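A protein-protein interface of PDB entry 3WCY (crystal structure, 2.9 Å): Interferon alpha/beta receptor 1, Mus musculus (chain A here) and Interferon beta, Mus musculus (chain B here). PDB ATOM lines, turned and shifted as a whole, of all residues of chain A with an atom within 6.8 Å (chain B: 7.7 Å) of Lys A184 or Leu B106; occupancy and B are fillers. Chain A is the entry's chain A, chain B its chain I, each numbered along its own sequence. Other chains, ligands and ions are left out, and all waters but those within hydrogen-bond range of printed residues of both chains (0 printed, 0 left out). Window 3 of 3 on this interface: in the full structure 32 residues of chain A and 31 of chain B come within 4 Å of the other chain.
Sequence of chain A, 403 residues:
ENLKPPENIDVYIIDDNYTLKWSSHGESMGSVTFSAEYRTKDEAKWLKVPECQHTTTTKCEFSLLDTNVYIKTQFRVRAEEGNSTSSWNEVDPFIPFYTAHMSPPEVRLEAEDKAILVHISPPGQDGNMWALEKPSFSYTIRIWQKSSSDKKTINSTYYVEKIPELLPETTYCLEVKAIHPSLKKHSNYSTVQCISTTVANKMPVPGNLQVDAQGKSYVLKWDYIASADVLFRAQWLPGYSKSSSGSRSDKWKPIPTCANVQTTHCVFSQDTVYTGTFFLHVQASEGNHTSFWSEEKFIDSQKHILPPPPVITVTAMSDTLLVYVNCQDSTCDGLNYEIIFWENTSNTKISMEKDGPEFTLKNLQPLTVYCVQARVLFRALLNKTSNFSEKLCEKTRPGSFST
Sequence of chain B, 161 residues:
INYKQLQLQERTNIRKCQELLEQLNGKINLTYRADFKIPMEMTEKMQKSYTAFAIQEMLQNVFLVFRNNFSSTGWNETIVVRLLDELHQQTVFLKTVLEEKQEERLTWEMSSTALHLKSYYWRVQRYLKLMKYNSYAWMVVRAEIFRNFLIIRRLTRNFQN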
ATOM      1  N   HIS A 180      -6.419 -24.042 -17.519  1.00  0.00           N
ATOM      2  CA  HIS A 180      -6.296 -23.819 -16.070  1.00  0.00           C
ATOM      3  C   HIS A 180      -7.175 -22.572 -15.791  1.00  0.00           C
ATOM      4  O   HIS A 180      -6.682 -21.445 -15.913  1.00  0.00           O
ATOM      5  CB  HIS A 180      -4.822 -23.573 -15.656  1.00  0.00           C
ATOM      6  CG  HIS A 180      -4.518 -23.822 -14.202  1.00  0.00           C
ATOM      7  ND1 HIS A 180      -5.475 -23.638 -13.205  1.00  0.00           N
ATOM      8  CD2 HIS A 180      -3.359 -24.213 -13.620  1.00  0.00           C
ATOM      9  CE1 HIS A 180      -4.871 -23.935 -12.065  1.00  0.00           C
ATOM     10  NE2 HIS A 180      -3.598 -24.285 -12.260  1.00  0.00           N
ATOM     11  N   PRO A 181      -8.493 -22.743 -15.502  1.00  0.00           N
ATOM     12  CA  PRO A 181      -9.373 -21.570 -15.352  1.00  0.00           C
ATOM     13  C   PRO A 181      -9.093 -20.610 -14.200  1.00  0.00           C
ATOM     14  O   PRO A 181      -9.670 -19.520 -14.184  1.00  0.00           O
ATOM     15  CB  PRO A 181     -10.777 -22.183 -15.268  1.00  0.00           C
ATOM     16  CG  PRO A 181     -10.561 -23.558 -14.772  1.00  0.00           C
ATOM     17  CD  PRO A 181      -9.262 -23.999 -15.374  1.00  0.00           C
ATOM     18  N   SER A 182      -8.222 -20.995 -13.247  1.00  0.00           N
ATOM     19  CA  SER A 182      -7.897 -20.155 -12.093  1.00  0.00           C
ATOM     20  C   SER A 182      -6.503 -19.524 -12.149  1.00  0.00           C
ATOM     21  O   SER A 182      -6.346 -18.370 -11.747  1.00  0.00           O
ATOM     22  CB  SER A 182      -8.103 -20.924 -10.791  1.00  0.00           C
ATOM     23  OG  SER A 182      -9.449 -21.356 -10.662  1.00  0.00           O
ATOM     24  N   LEU A 183      -5.499 -20.265 -12.650  1.00  0.00           N
ATOM     25  CA  LEU A 183      -4.121 -19.776 -12.732  1.00  0.00           C
ATOM     26  C   LEU A 183      -3.779 -19.116 -14.074  1.00  0.00           C
ATOM     27  O   LEU A 183      -2.631 -19.206 -14.523  1.00  0.00           O
ATOM     28  CB  LEU A 183      -3.124 -20.893 -12.382  1.00  0.00           C
ATOM     29  CG  LEU A 183      -1.800 -20.454 -11.766  1.00  0.00           C
ATOM     30  CD1 LEU A 183      -1.800 -20.661 -10.275  1.00  0.00           C
ATOM     31  CD2 LEU A 183      -0.645 -21.199 -12.388  1.00  0.00           C
ATOM     32  N   LYS A 184      -4.766 -18.430 -14.708  1.00  0.00           N
ATOM     33  CA  LYS A 184      -4.597 -17.677 -15.965  1.00  0.00           C
ATOM     34  C   LYS A 184      -4.230 -18.533 -17.217  1.00  0.00           C
ATOM     35  O   LYS A 184      -4.903 -18.421 -18.246  1.00  0.00           O
ATOM     36  CB  LYS A 184      -3.582 -16.534 -15.750  1.00  0.00           C
ATOM     37  CG  LYS A 184      -3.750 -15.314 -16.642  1.00  0.00           C
ATOM     38  CD  LYS A 184      -2.951 -14.112 -16.104  1.00  0.00           C
ATOM     39  CE  LYS A 184      -1.446 -14.309 -16.119  1.00  0.00           C
ATOM     40  NZ  LYS A 184      -0.730 -13.174 -15.488  1.00  0.00           N
ATOM     41  N   LYS A 185      -3.168 -19.364 -17.114  1.00  0.00           N
ATOM     42  CA  LYS A 185      -2.607 -20.226 -18.157  1.00  0.00           C
ATOM     43  C   LYS A 185      -3.575 -21.134 -18.936  1.00  0.00           C
ATOM     44  O   LYS A 185      -4.688 -21.417 -18.485  1.00  0.00           O
ATOM     45  CB  LYS A 185      -1.397 -21.009 -17.627  1.00  0.00           C
ATOM     46  CG  LYS A 185      -0.118 -20.180 -17.601  1.00  0.00           C
ATOM     47  CD  LYS A 185       0.315 -19.829 -16.184  1.00  0.00           C
ATOM     48  CE  LYS A 185       1.490 -20.657 -15.716  1.00  0.00           C
ATOM     49  NZ  LYS A 185       2.749 -20.292 -16.425  1.00  0.00           N
ATOM     50  N   HIS A 186      -3.127 -21.569 -20.129  1.00  0.00           N
ATOM     51  CA  HIS A 186      -3.856 -22.418 -21.078  1.00  0.00           C
ATOM     52  C   HIS A 186      -2.866 -23.218 -21.945  1.00  0.00           C
ATOM     53  O   HIS A 186      -1.664 -22.927 -21.951  1.00  0.00           O
ATOM     54  CB  HIS A 186      -4.804 -21.567 -21.950  1.00  0.00           C
ATOM     55  CG  HIS A 186      -4.131 -20.402 -22.606  1.00  0.00           C
ATOM     56  ND1 HIS A 186      -3.923 -19.211 -21.927  1.00  0.00           N
ATOM     57  CD2 HIS A 186      -3.617 -20.289 -23.852  1.00  0.00           C
ATOM     58  CE1 HIS A 186      -3.299 -18.416 -22.779  1.00  0.00           C
ATOM     59  NE2 HIS A 186      -3.094 -19.020 -23.951  1.00  0.00           N
ATOM     60  N   TYR B  50     -10.258 -14.801   0.013  1.00  0.00           N
ATOM     61  CA  TYR B  50      -9.077 -15.651   0.207  1.00  0.00           C
ATOM     62  C   TYR B  50      -9.358 -16.921   1.025  1.00  0.00           C
ATOM     63  O   TYR B  50      -8.727 -17.947   0.764  1.00  0.00           O
ATOM     64  CB  TYR B  50      -7.927 -14.837   0.849  1.00  0.00           C
ATOM     65  CG  TYR B  50      -7.128 -13.929  -0.075  1.00  0.00           C
ATOM     66  CD1 TYR B  50      -7.621 -13.559  -1.327  1.00  0.00           C
ATOM     67  CD2 TYR B  50      -5.892 -13.423   0.313  1.00  0.00           C
ATOM     68  CE1 TYR B  50      -6.890 -12.728  -2.175  1.00  0.00           C
ATOM     69  CE2 TYR B  50      -5.156 -12.585  -0.525  1.00  0.00           C
ATOM     70  CZ  TYR B  50      -5.662 -12.235  -1.767  1.00  0.00           C
ATOM     71  OH  TYR B  50      -4.946 -11.397  -2.588  1.00  0.00           O
ATOM     72  N   PHE B  53     -11.175 -19.710  -1.072  1.00  0.00           N
ATOM     73  CA  PHE B  53     -10.161 -20.340  -1.928  1.00  0.00           C
ATOM     74  C   PHE B  53      -9.260 -21.262  -1.117  1.00  0.00           C
ATOM     75  O   PHE B  53      -8.958 -22.367  -1.577  1.00  0.00           O
ATOM     76  CB  PHE B  53      -9.301 -19.317  -2.696  1.00  0.00           C
ATOM     77  CG  PHE B  53     -10.020 -18.209  -3.426  1.00  0.00           C
ATOM     78  CD1 PHE B  53     -11.024 -18.493  -4.345  1.00  0.00           C
ATOM     79  CD2 PHE B  53      -9.648 -16.887  -3.249  1.00  0.00           C
ATOM     80  CE1 PHE B  53     -11.691 -17.468  -5.012  1.00  0.00           C
ATOM     81  CE2 PHE B  53     -10.305 -15.861  -3.928  1.00  0.00           C
ATOM     82  CZ  PHE B  53     -11.329 -16.160  -4.794  1.00  0.00           C
ATOM     83  N   GLN B 102     -14.374 -13.437 -10.805  1.00  0.00           N
ATOM     84  CA  GLN B 102     -13.179 -13.956 -11.488  1.00  0.00           C
ATOM     85  C   GLN B 102     -11.854 -13.205 -11.240  1.00  0.00           C
ATOM     86  O   GLN B 102     -10.783 -13.773 -11.474  1.00  0.00           O
ATOM     87  CB  GLN B 102     -13.463 -14.167 -12.986  1.00  0.00           C
ATOM     88  CG  GLN B 102     -12.622 -15.260 -13.664  1.00  0.00           C
ATOM     89  CD  GLN B 102     -12.612 -16.590 -12.942  1.00  0.00           C
ATOM     90  OE1 GLN B 102     -13.655 -17.141 -12.562  1.00  0.00           O
ATOM     91  NE2 GLN B 102     -11.424 -17.143 -12.750  1.00  0.00           N
ATOM     92  N   GLU B 103     -11.919 -11.963 -10.733  1.00  0.00           N
ATOM     93  CA  GLU B 103     -10.719 -11.159 -10.491  1.00  0.00           C
ATOM     94  C   GLU B 103      -9.886 -11.562  -9.279  1.00  0.00           C
ATOM     95  O   GLU B 103      -8.688 -11.810  -9.442  1.00  0.00           O
ATOM     96  CB  GLU B 103     -11.016  -9.649 -10.501  1.00  0.00           C
ATOM     97  CG  GLU B 103     -11.356  -9.089 -11.875  1.00  0.00           C
ATOM     98  CD  GLU B 103     -10.354  -9.383 -12.977  1.00  0.00           C
ATOM     99  OE1 GLU B 103      -9.235  -8.822 -12.932  1.00  0.00           O
ATOM    100  OE2 GLU B 103     -10.680 -10.193 -13.875  1.00  0.00           O
ATOM    101  N   GLU B 104     -10.509 -11.616  -8.074  1.00  0.00           N
ATOM    102  CA  GLU B 104      -9.830 -11.942  -6.809  1.00  0.00           C
ATOM    103  C   GLU B 104      -9.143 -13.307  -6.700  1.00  0.00           C
ATOM    104  O   GLU B 104      -8.178 -13.429  -5.944  1.00  0.00           O
ATOM    105  CB  GLU B 104     -10.651 -11.569  -5.553  1.00  0.00           C
ATOM    106  CG  GLU B 104     -12.041 -12.171  -5.465  1.00  0.00           C
ATOM    107  CD  GLU B 104     -13.140 -11.291  -6.023  1.00  0.00           C
ATOM    108  OE1 GLU B 104     -13.847 -10.645  -5.216  1.00  0.00           O
ATOM    109  OE2 GLU B 104     -13.296 -11.242  -7.264  1.00  0.00           O
ATOM    110  N   ARG B 105      -9.605 -14.320  -7.464  1.00  0.00           N
ATOM    111  CA  ARG B 105      -8.975 -15.652  -7.474  1.00  0.00           C
ATOM    112  C   ARG B 105      -7.610 -15.615  -8.147  1.00  0.00           C
ATOM    113  O   ARG B 105      -6.706 -16.342  -7.726  1.00  0.00           O
ATOM    114  CB  ARG B 105      -9.873 -16.749  -8.087  1.00  0.00           C
ATOM    115  CG  ARG B 105     -10.633 -16.336  -9.341  1.00  0.00           C
ATOM    116  CD  ARG B 105     -12.116 -16.704  -9.308  1.00  0.00           C
ATOM    117  NE  ARG B 105     -12.833 -16.388  -8.059  1.00  0.00           N
ATOM    118  CZ  ARG B 105     -13.119 -15.166  -7.602  1.00  0.00           C
ATOM    119  NH1 ARG B 105     -12.681 -14.090  -8.242  1.00  0.00           N
ATOM    120  NH2 ARG B 105     -13.801 -15.016  -6.474  1.00  0.00           N
ATOM    121  N   LEU B 106      -7.458 -14.740  -9.172  1.00  0.00           N
ATOM    122  CA  LEU B 106      -6.200 -14.539  -9.883  1.00  0.00           C
ATOM    123  C   LEU B 106      -5.186 -13.922  -8.919  1.00  0.00           C
ATOM    124  O   LEU B 106      -4.042 -14.380  -8.871  1.00  0.00           O
ATOM    125  CB  LEU B 106      -6.404 -13.641 -11.108  1.00  0.00           C
ATOM    126  CG  LEU B 106      -5.286 -13.681 -12.146  1.00  0.00           C
ATOM    127  CD1 LEU B 106      -5.573 -14.714 -13.199  1.00  0.00           C
ATOM    128  CD2 LEU B 106      -5.091 -12.321 -12.791  1.00  0.00           C
ATOM    129  N   THR B 107      -5.629 -12.927  -8.110  1.00  0.00           N
ATOM    130  CA  THR B 107      -4.814 -12.260  -7.087  1.00  0.00           C
ATOM    131  C   THR B 107      -4.397 -13.283  -6.025  1.00  0.00           C
ATOM    132  O   THR B 107      -3.261 -13.242  -5.548  1.00  0.00           O
ATOM    133  CB  THR B 107      -5.580 -11.087  -6.452  1.00  0.00           C
ATOM    134  OG1 THR B 107      -6.353 -10.411  -7.445  1.00  0.00           O
ATOM    135  CG2 THR B 107      -4.661 -10.100  -5.750  1.00  0.00           C
ATOM    136  N   TRP B 108      -5.314 -14.214  -5.683  1.00  0.00           N
ATOM    137  CA  TRP B 108      -5.041 -15.255  -4.706  1.00  0.00           C
ATOM    138  C   TRP B 108      -4.057 -16.297  -5.211  1.00  0.00           C
ATOM    139  O   TRP B 108      -3.275 -16.807  -4.411  1.00  0.00           O
ATOM    140  CB  TRP B 108      -6.313 -15.910  -4.179  1.00  0.00           C
ATOM    141  CG  TRP B 108      -6.033 -16.861  -3.052  1.00  0.00           C
ATOM    142  CD1 TRP B 108      -5.755 -16.539  -1.755  1.00  0.00           C
ATOM    143  CD2 TRP B 108      -5.861 -18.277  -3.160  1.00  0.00           C
ATOM    144  NE1 TRP B 108      -5.479 -17.676  -1.033  1.00  0.00           N
ATOM    145  CE2 TRP B 108      -5.536 -18.759  -1.872  1.00  0.00           C
ATOM    146  CE3 TRP B 108      -5.989 -19.192  -4.212  1.00  0.00           C
ATOM    147  CZ2 TRP B 108      -5.360 -20.119  -1.606  1.00  0.00           C
ATOM    148  CZ3 TRP B 108      -5.807 -20.539  -3.950  1.00  0.00           C
ATOM    149  CH2 TRP B 108      -5.489 -20.990  -2.662  1.00  0.00           C
ATOM    150  N   GLU B 109      -4.092 -16.624  -6.521  1.00  0.00           N
ATOM    151  CA  GLU B 109      -3.182 -17.613  -7.101  1.00  0.00           C
ATOM    152  C   GLU B 109      -1.741 -17.093  -7.186  1.00  0.00           C
ATOM    153  O   GLU B 109      -0.797 -17.876  -7.089  1.00  0.00           O
ATOM    154  CB  GLU B 109      -3.687 -18.108  -8.459  1.00  0.00           C
ATOM    155  CG  GLU B 109      -4.911 -19.015  -8.383  1.00  0.00           C
ATOM    156  CD  GLU B 109      -4.724 -20.487  -8.048  1.00  0.00           C
ATOM    157  OE1 GLU B 109      -5.640 -21.279  -8.370  1.00  0.00           O
ATOM    158  OE2 GLU B 109      -3.686 -20.852  -7.449  1.00  0.00           O
ATOM    159  N   MET B 110      -1.580 -15.765  -7.314  1.00  0.00           N
ATOM    160  CA  MET B 110      -0.272 -15.105  -7.383  1.00  0.00           C
ATOM    161  C   MET B 110       0.233 -14.682  -5.995  1.00  0.00           C
ATOM    162  O   MET B 110       1.324 -14.105  -5.884  1.00  0.00           O
ATOM    163  CB  MET B 110      -0.300 -13.921  -8.370  1.00  0.00           C
ATOM    164  CG  MET B 110      -0.671 -14.312  -9.795  1.00  0.00           C
ATOM    165  SD  MET B 110       0.429 -15.550 -10.533  1.00  0.00           S
ATOM    166  CE  MET B 110      -0.698 -16.925 -10.691  1.00  0.00           C
ATOM    167  N   SER B 111      -0.556 -14.995  -4.938  1.00  0.00           N
ATOM    168  CA  SER B 111      -0.239 -14.707  -3.539  1.00  0.00           C
ATOM    169  C   SER B 111       0.885 -15.595  -3.028  1.00  0.00           C
ATOM    170  O   SER B 111       1.026 -16.732  -3.479  1.00  0.00           O
ATOM    171  CB  SER B 111      -1.461 -14.947  -2.657  1.00  0.00           C
ATOM    172  OG  SER B 111      -2.577 -14.193  -3.092  1.00  0.00           O
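ND1 of His A180 is in hydrogen-bond range of N of Leu A183 (3.4 Å).
Printed residues of chain B within 4 Å of Pro A181: Gln B102. Of the printed residues of chain B, Ser A182 touches Glu B109. Printed residues of chain B within 4 Å of Leu A183: Glu B109 (3.4 Å) and Met B110 (3.9 Å). Of the printed residues of chain B, Lys A184 touches Leu B106. Of the printed residues of chain A, Leu B106 touches Lys A184 (3.7 Å). Of the printed residues of chain A, Glu B109 touches Ser A182 and Leu A183. Of the printed residues of chain A, Met B110 touches Leu A183. The nearest printed residue of chain A that does not touch Leu B106 is Ser A182 (4.01 Å).
Of the 7 printed residues of chain A, 4 touch a printed residue of chain B. Printed residues of chain A that touch a printed residue of chain B: Pro A181, Ser A182, Leu A183 and Lys A184. Hydrophobic or aromatic side chains of chain A that line the printed part of chain B: Leu A183. Hydrophobic or aromatic side chains of chain B that line the printed part of chain A: Leu B106 and Met B110. Among the printed residues, 5 pairs touch across the chains. Among the printed residues, no Asp or Glu carboxylate lies within 4 Å of a Lys or Arg side-chain nitrogen of the other chain.
NE2 of Gln B102 sits at hydrogen-bond distance from O of Pro A181, 3.3 Å away.
Ser A182 touches Glu B109. OE2 of Glu B109 touches CD1 of Leu A183, at 3.4 Å. Leu A183 touches Met B110 (CG to CE, 3.9 Å). CB of Lys A184 touches CD1 of Leu B106, at 3.7 Å.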
